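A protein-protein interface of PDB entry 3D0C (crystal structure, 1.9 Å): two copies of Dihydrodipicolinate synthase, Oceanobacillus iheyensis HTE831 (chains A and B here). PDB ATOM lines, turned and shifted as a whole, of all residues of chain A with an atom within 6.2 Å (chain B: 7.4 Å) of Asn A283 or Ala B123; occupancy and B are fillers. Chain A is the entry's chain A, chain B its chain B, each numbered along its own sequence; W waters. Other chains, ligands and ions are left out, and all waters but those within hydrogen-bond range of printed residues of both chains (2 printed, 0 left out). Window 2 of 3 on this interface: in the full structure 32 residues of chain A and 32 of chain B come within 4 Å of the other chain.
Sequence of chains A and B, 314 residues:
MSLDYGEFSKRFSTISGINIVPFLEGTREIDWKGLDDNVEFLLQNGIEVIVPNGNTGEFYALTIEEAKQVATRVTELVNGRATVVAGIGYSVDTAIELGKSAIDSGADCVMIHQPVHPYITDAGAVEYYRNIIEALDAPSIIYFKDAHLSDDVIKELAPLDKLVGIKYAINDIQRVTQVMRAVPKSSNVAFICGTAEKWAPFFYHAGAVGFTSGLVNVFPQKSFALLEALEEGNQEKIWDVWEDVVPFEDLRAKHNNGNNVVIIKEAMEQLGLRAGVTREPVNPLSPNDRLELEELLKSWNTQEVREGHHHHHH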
ATOM      1  N   ARG A  28      34.251 -23.765   0.992  1.00  0.00           N
ATOM      2  CA  ARG A  28      34.432 -23.251  -0.362  1.00  0.00           C
ATOM      3  C   ARG A  28      35.151 -21.911  -0.385  1.00  0.00           C
ATOM      4  O   ARG A  28      35.157 -21.230  -1.412  1.00  0.00           O
ATOM      5  CB  ARG A  28      33.087 -23.102  -1.080  1.00  0.00           C
ATOM      6  CG  ARG A  28      32.295 -24.395  -1.275  1.00  0.00           C
ATOM      7  CD  ARG A  28      31.230 -24.191  -2.351  1.00  0.00           C
ATOM      8  NE  ARG A  28      30.192 -25.220  -2.368  1.00  0.00           N
ATOM      9  CZ  ARG A  28      30.171 -26.271  -3.186  1.00  0.00           C
ATOM     10  NH1 ARG A  28      31.140 -26.457  -4.074  1.00  0.00           N
ATOM     11  NH2 ARG A  28      29.157 -27.125  -3.133  1.00  0.00           N
ATOM     12  N   VAL A 262      35.836 -28.140 -13.836  1.00  0.00           N
ATOM     13  CA  VAL A 262      35.907 -29.332 -12.994  1.00  0.00           C
ATOM     14  C   VAL A 262      36.857 -30.374 -13.579  1.00  0.00           C
ATOM     15  O   VAL A 262      37.503 -31.119 -12.839  1.00  0.00           O
ATOM     16  CB  VAL A 262      34.499 -29.947 -12.760  1.00  0.00           C
ATOM     17  CG1 VAL A 262      33.836 -30.260 -14.077  1.00  0.00           C
ATOM     18  CG2 VAL A 262      34.610 -31.201 -11.890  1.00  0.00           C
ATOM     19  N   GLU A 266      39.922 -31.739 -11.241  1.00  0.00           N
ATOM     20  CA  GLU A 266      40.018 -33.149 -10.909  1.00  0.00           C
ATOM     21  C   GLU A 266      41.301 -33.717 -11.499  1.00  0.00           C
ATOM     22  O   GLU A 266      41.932 -34.587 -10.902  1.00  0.00           O
ATOM     23  CB  GLU A 266      38.786 -33.910 -11.405  1.00  0.00           C
ATOM     24  CG  GLU A 266      37.566 -33.647 -10.543  1.00  0.00           C
ATOM     25  CD  GLU A 266      36.566 -34.786 -10.559  1.00  0.00           C
ATOM     26  OE1 GLU A 266      36.988 -35.952 -10.720  1.00  0.00           O
ATOM     27  OE2 GLU A 266      35.359 -34.516 -10.385  1.00  0.00           O
ATOM     28  N   THR A 278      35.076 -27.401  -7.566  1.00  0.00           N
ATOM     29  CA  THR A 278      34.480 -26.203  -8.151  1.00  0.00           C
ATOM     30  C   THR A 278      33.325 -25.685  -7.290  1.00  0.00           C
ATOM     31  O   THR A 278      32.693 -26.452  -6.559  1.00  0.00           O
ATOM     32  CB  THR A 278      33.929 -26.498  -9.573  1.00  0.00           C
ATOM     33  OG1 THR A 278      33.060 -27.641  -9.526  1.00  0.00           O
ATOM     34  CG2 THR A 278      35.066 -26.768 -10.551  1.00  0.00           C
ATOM     35  N   ARG A 279      33.056 -24.382  -7.368  1.00  0.00           N
ATOM     36  CA  ARG A 279      31.941 -23.796  -6.626  1.00  0.00           C
ATOM     37  C   ARG A 279      30.664 -24.003  -7.431  1.00  0.00           C
ATOM     38  O   ARG A 279      30.716 -24.381  -8.606  1.00  0.00           O
ATOM     39  CB  ARG A 279      32.140 -22.295  -6.420  1.00  0.00           C
ATOM     40  CG  ARG A 279      33.016 -21.920  -5.240  1.00  0.00           C
ATOM     41  CD  ARG A 279      32.945 -20.425  -4.958  1.00  0.00           C
ATOM     42  NE  ARG A 279      33.736 -20.060  -3.789  1.00  0.00           N
ATOM     43  CZ  ARG A 279      33.852 -18.825  -3.311  1.00  0.00           C
ATOM     44  NH1 ARG A 279      33.224 -17.816  -3.902  1.00  0.00           N
ATOM     45  NH2 ARG A 279      34.595 -18.600  -2.236  1.00  0.00           N
ATOM     46  N   GLU A 280      29.520 -23.767  -6.794  1.00  0.00           N
ATOM     47  CA  GLU A 280      28.235 -23.881  -7.472  1.00  0.00           C
ATOM     48  C   GLU A 280      28.328 -22.852  -8.605  1.00  0.00           C
ATOM     49  O   GLU A 280      28.982 -21.825  -8.445  1.00  0.00           O
ATOM     50  CB  GLU A 280      27.088 -23.487  -6.524  1.00  0.00           C
ATOM     51  CG  GLU A 280      27.087 -24.203  -5.164  1.00  0.00           C
ATOM     52  CD  GLU A 280      27.877 -23.462  -4.090  1.00  0.00           C
ATOM     53  OE1 GLU A 280      29.071 -23.172  -4.305  1.00  0.00           O
ATOM     54  OE2 GLU A 280      27.300 -23.169  -3.020  1.00  0.00           O
ATOM     55  N   PRO A 281      27.664 -23.099  -9.751  1.00  0.00           N
ATOM     56  CA  PRO A 281      26.795 -24.225 -10.092  1.00  0.00           C
ATOM     57  C   PRO A 281      27.461 -25.427 -10.785  1.00  0.00           C
ATOM     58  O   PRO A 281      26.878 -25.993 -11.709  1.00  0.00           O
ATOM     59  CB  PRO A 281      25.752 -23.569 -10.988  1.00  0.00           C
ATOM     60  CG  PRO A 281      26.631 -22.669 -11.836  1.00  0.00           C
ATOM     61  CD  PRO A 281      27.643 -22.090 -10.832  1.00  0.00           C
ATOM     62  N   VAL A 282      28.665 -25.807 -10.366  1.00  0.00           N
ATOM     63  CA  VAL A 282      29.316 -26.979 -10.954  1.00  0.00           C
ATOM     64  C   VAL A 282      29.722 -27.929  -9.825  1.00  0.00           C
ATOM     65  O   VAL A 282      30.390 -27.535  -8.878  1.00  0.00           O
ATOM     66  CB  VAL A 282      30.572 -26.605 -11.800  1.00  0.00           C
ATOM     67  CG1 VAL A 282      31.243 -27.882 -12.336  1.00  0.00           C
ATOM     68  CG2 VAL A 282      30.159 -25.718 -12.988  1.00  0.00           C
ATOM     69  N   ASN A 283      29.293 -29.179  -9.924  1.00  0.00           N
ATOM     70  CA  ASN A 283      29.618 -30.166  -8.904  1.00  0.00           C
ATOM     71  C   ASN A 283      30.722 -31.060  -9.443  1.00  0.00           C
ATOM     72  O   ASN A 283      31.245 -30.812 -10.530  1.00  0.00           O
ATOM     73  CB  ASN A 283      28.367 -30.974  -8.571  1.00  0.00           C
ATOM     74  CG  ASN A 283      27.795 -30.624  -7.207  1.00  0.00           C
ATOM     75  OD1 ASN A 283      28.026 -29.533  -6.679  1.00  0.00           O
ATOM     76  ND2 ASN A 283      27.038 -31.552  -6.634  1.00  0.00           N
ATOM     77  N   PRO A 284      31.106 -32.104  -8.692  1.00  0.00           N
ATOM     78  CA  PRO A 284      32.167 -32.997  -9.175  1.00  0.00           C
ATOM     79  C   PRO A 284      31.761 -33.692 -10.477  1.00  0.00           C
ATOM     80  O   PRO A 284      30.584 -33.726 -10.822  1.00  0.00           O
ATOM     81  CB  PRO A 284      32.332 -33.985  -8.021  1.00  0.00           C
ATOM     82  CG  PRO A 284      31.985 -33.149  -6.816  1.00  0.00           C
ATOM     83  CD  PRO A 284      30.758 -32.410  -7.292  1.00  0.00           C
ATOM     84  N   LEU A 285      32.732 -34.251 -11.195  1.00  0.00           N
ATOM     85  CA  LEU A 285      32.447 -34.946 -12.450  1.00  0.00           C
ATOM     86  C   LEU A 285      31.469 -36.102 -12.260  1.00  0.00           C
ATOM     87  O   LEU A 285      31.353 -36.663 -11.165  1.00  0.00           O
ATOM     88  CB  LEU A 285      33.737 -35.509 -13.053  1.00  0.00           C
ATOM     89  CG  LEU A 285      34.851 -34.547 -13.461  1.00  0.00           C
ATOM     90  CD1 LEU A 285      36.057 -35.346 -13.934  1.00  0.00           C
ATOM     91  CD2 LEU A 285      34.360 -33.629 -14.561  1.00  0.00           C
ATOM     92  N   ILE B 120      27.938 -24.774 -16.134  1.00  0.00           N
ATOM     93  CA  ILE B 120      26.965 -25.251 -15.160  1.00  0.00           C
ATOM     94  C   ILE B 120      26.496 -26.674 -15.463  1.00  0.00           C
ATOM     95  O   ILE B 120      26.356 -27.058 -16.622  1.00  0.00           O
ATOM     96  CB  ILE B 120      25.741 -24.281 -15.127  1.00  0.00           C
ATOM     97  CG1 ILE B 120      24.687 -24.763 -14.131  1.00  0.00           C
ATOM     98  CG2 ILE B 120      25.144 -24.145 -16.522  1.00  0.00           C
ATOM     99  CD1 ILE B 120      23.594 -23.734 -13.869  1.00  0.00           C
ATOM    100  N   THR B 121      26.282 -27.467 -14.414  1.00  0.00           N
ATOM    101  CA  THR B 121      25.794 -28.834 -14.583  1.00  0.00           C
ATOM    102  C   THR B 121      24.518 -29.009 -13.768  1.00  0.00           C
ATOM    103  O   THR B 121      24.219 -28.203 -12.878  1.00  0.00           O
ATOM    104  CB  THR B 121      26.806 -29.887 -14.098  1.00  0.00           C
ATOM    105  OG1 THR B 121      27.022 -29.724 -12.691  1.00  0.00           O
ATOM    106  CG2 THR B 121      28.130 -29.751 -14.839  1.00  0.00           C
ATOM    107  N   ASP B 122      23.772 -30.064 -14.073  1.00  0.00           N
ATOM    108  CA  ASP B 122      22.532 -30.346 -13.363  1.00  0.00           C
ATOM    109  C   ASP B 122      22.789 -30.418 -11.868  1.00  0.00           C
ATOM    110  O   ASP B 122      22.157 -29.708 -11.088  1.00  0.00           O
ATOM    111  CB  ASP B 122      21.926 -31.667 -13.842  1.00  0.00           C
ATOM    112  CG  ASP B 122      21.393 -31.584 -15.260  1.00  0.00           C
ATOM    113  OD1 ASP B 122      20.864 -30.514 -15.630  1.00  0.00           O
ATOM    114  OD2 ASP B 122      21.486 -32.590 -15.998  1.00  0.00           O
ATOM    115  N   ALA B 123      23.729 -31.269 -11.468  1.00  0.00           N
ATOM    116  CA  ALA B 123      24.049 -31.419 -10.054  1.00  0.00           C
ATOM    117  C   ALA B 123      24.467 -30.086  -9.422  1.00  0.00           C
ATOM    118  O   ALA B 123      23.994 -29.732  -8.341  1.00  0.00           O
ATOM    119  CB  ALA B 123      25.152 -32.465  -9.871  1.00  0.00           C
ATOM    120  N   GLY B 124      25.344 -29.350 -10.102  1.00  0.00           N
ATOM    121  CA  GLY B 124      25.802 -28.075  -9.573  1.00  0.00           C
ATOM    122  C   GLY B 124      24.692 -27.047  -9.492  1.00  0.00           C
ATOM    123  O   GLY B 124      24.702 -26.172  -8.612  1.00  0.00           O
ATOM    124  N   ALA B 125      23.741 -27.153 -10.420  1.00  0.00           N
ATOM    125  CA  ALA B 125      22.599 -26.248 -10.486  1.00  0.00           C
ATOM    126  C   ALA B 125      21.735 -26.466  -9.254  1.00  0.00           C
ATOM    127  O   ALA B 125      21.302 -25.516  -8.607  1.00  0.00           O
ATOM    128  CB  ALA B 125      21.784 -26.520 -11.747  1.00  0.00           C
ATOM    129  N   VAL B 126      21.482 -27.728  -8.933  1.00  0.00           N
ATOM    130  CA  VAL B 126      20.681 -28.040  -7.765  1.00  0.00           C
ATOM    131  C   VAL B 126      21.311 -27.454  -6.503  1.00  0.00           C
ATOM    132  O   VAL B 126      20.615 -26.869  -5.681  1.00  0.00           O
ATOM    133  CB  VAL B 126      20.508 -29.561  -7.605  1.00  0.00           C
ATOM    134  CG1 VAL B 126      19.831 -29.877  -6.285  1.00  0.00           C
ATOM    135  CG2 VAL B 126      19.690 -30.097  -8.768  1.00  0.00           C
ATOM    136  N   GLU B 127      22.625 -27.605  -6.351  1.00  0.00           N
ATOM    137  CA  GLU B 127      23.318 -27.063  -5.181  1.00  0.00           C
ATOM    138  C   GLU B 127      23.193 -25.544  -5.134  1.00  0.00           C
ATOM    139  O   GLU B 127      22.883 -24.959  -4.088  1.00  0.00           O
ATOM    140  CB  GLU B 127      24.803 -27.441  -5.208  1.00  0.00           C
ATOM    141  CG  GLU B 127      25.062 -28.916  -5.010  1.00  0.00           C
ATOM    142  CD  GLU B 127      24.432 -29.440  -3.733  1.00  0.00           C
ATOM    143  OE1 GLU B 127      24.780 -28.928  -2.647  1.00  0.00           O
ATOM    144  OE2 GLU B 127      23.588 -30.360  -3.822  1.00  0.00           O
ATOM    145  N   TYR B 128      23.451 -24.909  -6.273  1.00  0.00           N
ATOM    146  CA  TYR B 128      23.361 -23.459  -6.387  1.00  0.00           C
ATOM    147  C   TYR B 128      21.980 -22.991  -5.923  1.00  0.00           C
ATOM    148  O   TYR B 128      21.867 -22.149  -5.032  1.00  0.00           O
ATOM    149  CB  TYR B 128      23.589 -23.042  -7.844  1.00  0.00           C
ATOM    150  CG  TYR B 128      23.430 -21.561  -8.120  1.00  0.00           C
ATOM    151  CD1 TYR B 128      24.463 -20.663  -7.856  1.00  0.00           C
ATOM    152  CD2 TYR B 128      22.243 -21.059  -8.655  1.00  0.00           C
ATOM    153  CE1 TYR B 128      24.317 -19.298  -8.121  1.00  0.00           C
ATOM    154  CE2 TYR B 128      22.086 -19.701  -8.920  1.00  0.00           C
ATOM    155  CZ  TYR B 128      23.127 -18.825  -8.652  1.00  0.00           C
ATOM    156  OH  TYR B 128      22.983 -17.481  -8.914  1.00  0.00           O
ATOM    157  N   TYR B 129      20.932 -23.546  -6.523  1.00  0.00           N
ATOM    158  CA  TYR B 129      19.565 -23.164  -6.172  1.00  0.00           C
ATOM    159  C   TYR B 129      19.207 -23.473  -4.723  1.00  0.00           C
ATOM    160  O   TYR B 129      18.671 -22.627  -4.004  1.00  0.00           O
ATOM    161  CB  TYR B 129      18.569 -23.870  -7.093  1.00  0.00           C
ATOM    162  CG  TYR B 129      18.589 -23.373  -8.519  1.00  0.00           C
ATOM    163  CD1 TYR B 129      18.442 -22.015  -8.801  1.00  0.00           C
ATOM    164  CD2 TYR B 129      18.725 -24.258  -9.585  1.00  0.00           C
ATOM    165  CE1 TYR B 129      18.428 -21.551 -10.111  1.00  0.00           C
ATOM    166  CE2 TYR B 129      18.711 -23.801 -10.900  1.00  0.00           C
ATOM    167  CZ  TYR B 129      18.562 -22.448 -11.154  1.00  0.00           C
ATOM    168  OH  TYR B 129      18.548 -21.994 -12.449  1.00  0.00           O
ATOM    169  N   ARG B 130      19.502 -24.697  -4.301  1.00  0.00           N
ATOM    170  CA  ARG B 130      19.203 -25.128  -2.946  1.00  0.00           C
ATOM    171  C   ARG B 130      19.855 -24.199  -1.924  1.00  0.00           C
ATOM    172  O   ARG B 130      19.201 -23.733  -0.988  1.00  0.00           O
ATOM    173  CB  ARG B 130      19.711 -26.553  -2.728  1.00  0.00           C
ATOM    174  CG  ARG B 130      19.161 -27.201  -1.482  1.00  0.00           C
ATOM    175  CD  ARG B 130      19.933 -28.456  -1.120  1.00  0.00           C
ATOM    176  NE  ARG B 130      19.919 -29.468  -2.175  1.00  0.00           N
ATOM    177  CZ  ARG B 130      18.824 -30.079  -2.615  1.00  0.00           C
ATOM    178  NH1 ARG B 130      17.639 -29.784  -2.100  1.00  0.00           N
ATOM    179  NH2 ARG B 130      18.919 -31.004  -3.559  1.00  0.00           N
ATOM    180  N   LEU B 149      20.097 -27.806 -19.479  1.00  0.00           N
ATOM    181  CA  LEU B 149      19.911 -28.398 -18.160  1.00  0.00           C
ATOM    182  C   LEU B 149      18.678 -29.291 -18.203  1.00  0.00           C
ATOM    183  O   LEU B 149      17.708 -28.999 -18.910  1.00  0.00           O
ATOM    184  CB  LEU B 149      19.731 -27.321 -17.082  1.00  0.00           C
ATOM    185  CG  LEU B 149      20.970 -26.497 -16.729  1.00  0.00           C
ATOM    186  CD1 LEU B 149      20.650 -25.566 -15.565  1.00  0.00           C
ATOM    187  CD2 LEU B 149      22.119 -27.441 -16.369  1.00  0.00           C
ATOM    188  N   VAL B 153      16.266 -31.116 -12.565  1.00  0.00           N
ATOM    189  CA  VAL B 153      16.728 -30.105 -11.623  1.00  0.00           C
ATOM    190  C   VAL B 153      15.514 -29.559 -10.884  1.00  0.00           C
ATOM    191  O   VAL B 153      15.532 -29.408  -9.665  1.00  0.00           O
ATOM    192  CB  VAL B 153      17.444 -28.940 -12.363  1.00  0.00           C
ATOM    193  CG1 VAL B 153      17.811 -27.823 -11.382  1.00  0.00           C
ATOM    194  CG2 VAL B 153      18.687 -29.464 -13.064  1.00  0.00           C
ATOM    195  N   GLU B 156      13.726 -32.223  -8.554  1.00  0.00           N
ATOM    196  CA  GLU B 156      14.430 -32.436  -7.299  1.00  0.00           C
ATOM    197  C   GLU B 156      14.216 -31.295  -6.308  1.00  0.00           C
ATOM    198  O   GLU B 156      14.193 -31.514  -5.100  1.00  0.00           O
ATOM    199  CB  GLU B 156      15.924 -32.624  -7.574  1.00  0.00           C
ATOM    200  CG  GLU B 156      16.813 -32.548  -6.346  1.00  0.00           C
ATOM    201  CD  GLU B 156      18.162 -33.205  -6.571  1.00  0.00           C
ATOM    202  OE1 GLU B 156      18.710 -33.063  -7.685  1.00  0.00           O
ATOM    203  OE2 GLU B 156      18.678 -33.854  -5.637  1.00  0.00           O
HETATM  204  O   HOH W   1      28.641 -31.641 -11.776  1.00  0.00           O
HETATM  205  O   HOH W   2      26.425 -27.280  -1.195  1.00  0.00           O
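The side-chain carboxylate of Glu A280 lies within salt-bridge range of the guanidinium group of Arg A28, 3.0 Å away.
The backbone carbonyl oxygen of Val A282 is in hydrogen-bond range of the side-chain hydroxyl of Thr A278, 2.7 Å away.
OG1 of Thr B121 lies within hydrogen-bond range of N of Gly B124.
Of the 14 printed residues of chain B, 7 touch a printed residue of chain A.
Printed residues of chain A that touch a printed residue of chain B: Glu A280, Pro A281, Val A282 and Asn A283.
Among the printed residues, 14 pairs touch across the chains.
Among the printed residues, no Asp or Glu carboxylate lies within 4 Å of a Lys or Arg side-chain nitrogen of the other chain.
Among the printed residues, pairs that only touch across the chains: Pro A281 with Gly B124, Asn A283 with Glu B127, Pro A281 with Ile B120, Pro A281 with Ala B125, Asn A283 with Thr B121, Asn A283 with Gly B124, Glu A280 with Tyr B128, Val A282 with Gly B124, Asn A283 with Ala B123, Pro A281 with Tyr B128, Val A282 with Ile B120, Glu A280 with Glu B127 and Val A282 with Thr B121.
No position is printed for both chains.
Of the 14 pairs that touch across the chains among the printed residues, none has its exchanged pair printed and touching as well.
Asn A283 touches just these residues of chain B: Thr B121 (3.6 Å), Ala B123 (3.8 Å), Gly B124 (3.7 Å) and Glu B127 (3.5 Å).
Printed residues of chain A within 4 Å of Tyr B128: Glu A280 (3.7 Å) and Pro A281 (3.9 Å).
Printed residues of chain B within 4 Å of Glu A280: Glu B127 and Tyr B128.
Glu B156 touches none of the printed residues of chain A.
The nearest residue of chain B that does not touch Asn A283 is Ala B125 (5.9 Å).
The nearest printed residue of chain A that does not touch Thr B121 is Pro A284 (5.7 Å).
The backbone carbonyl oxygen (O) of Pro A281 is in hydrogen-bond range of the backbone NH (N) of Thr B121 (3.1 Å).
Water W1 lies within hydrogen-bond range of the side-chain hydroxyl of Thr B121 (2.7 Å), the backbone carbonyl oxygen of Asn A283 (3.0 Å) and the backbone carbonyl oxygen of Pro A284 (3.0 Å).
Water W2 lies within hydrogen-bond range of OE1 of Glu B127 (2.7 Å) and NH2 of Arg A28 (3.4 Å).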
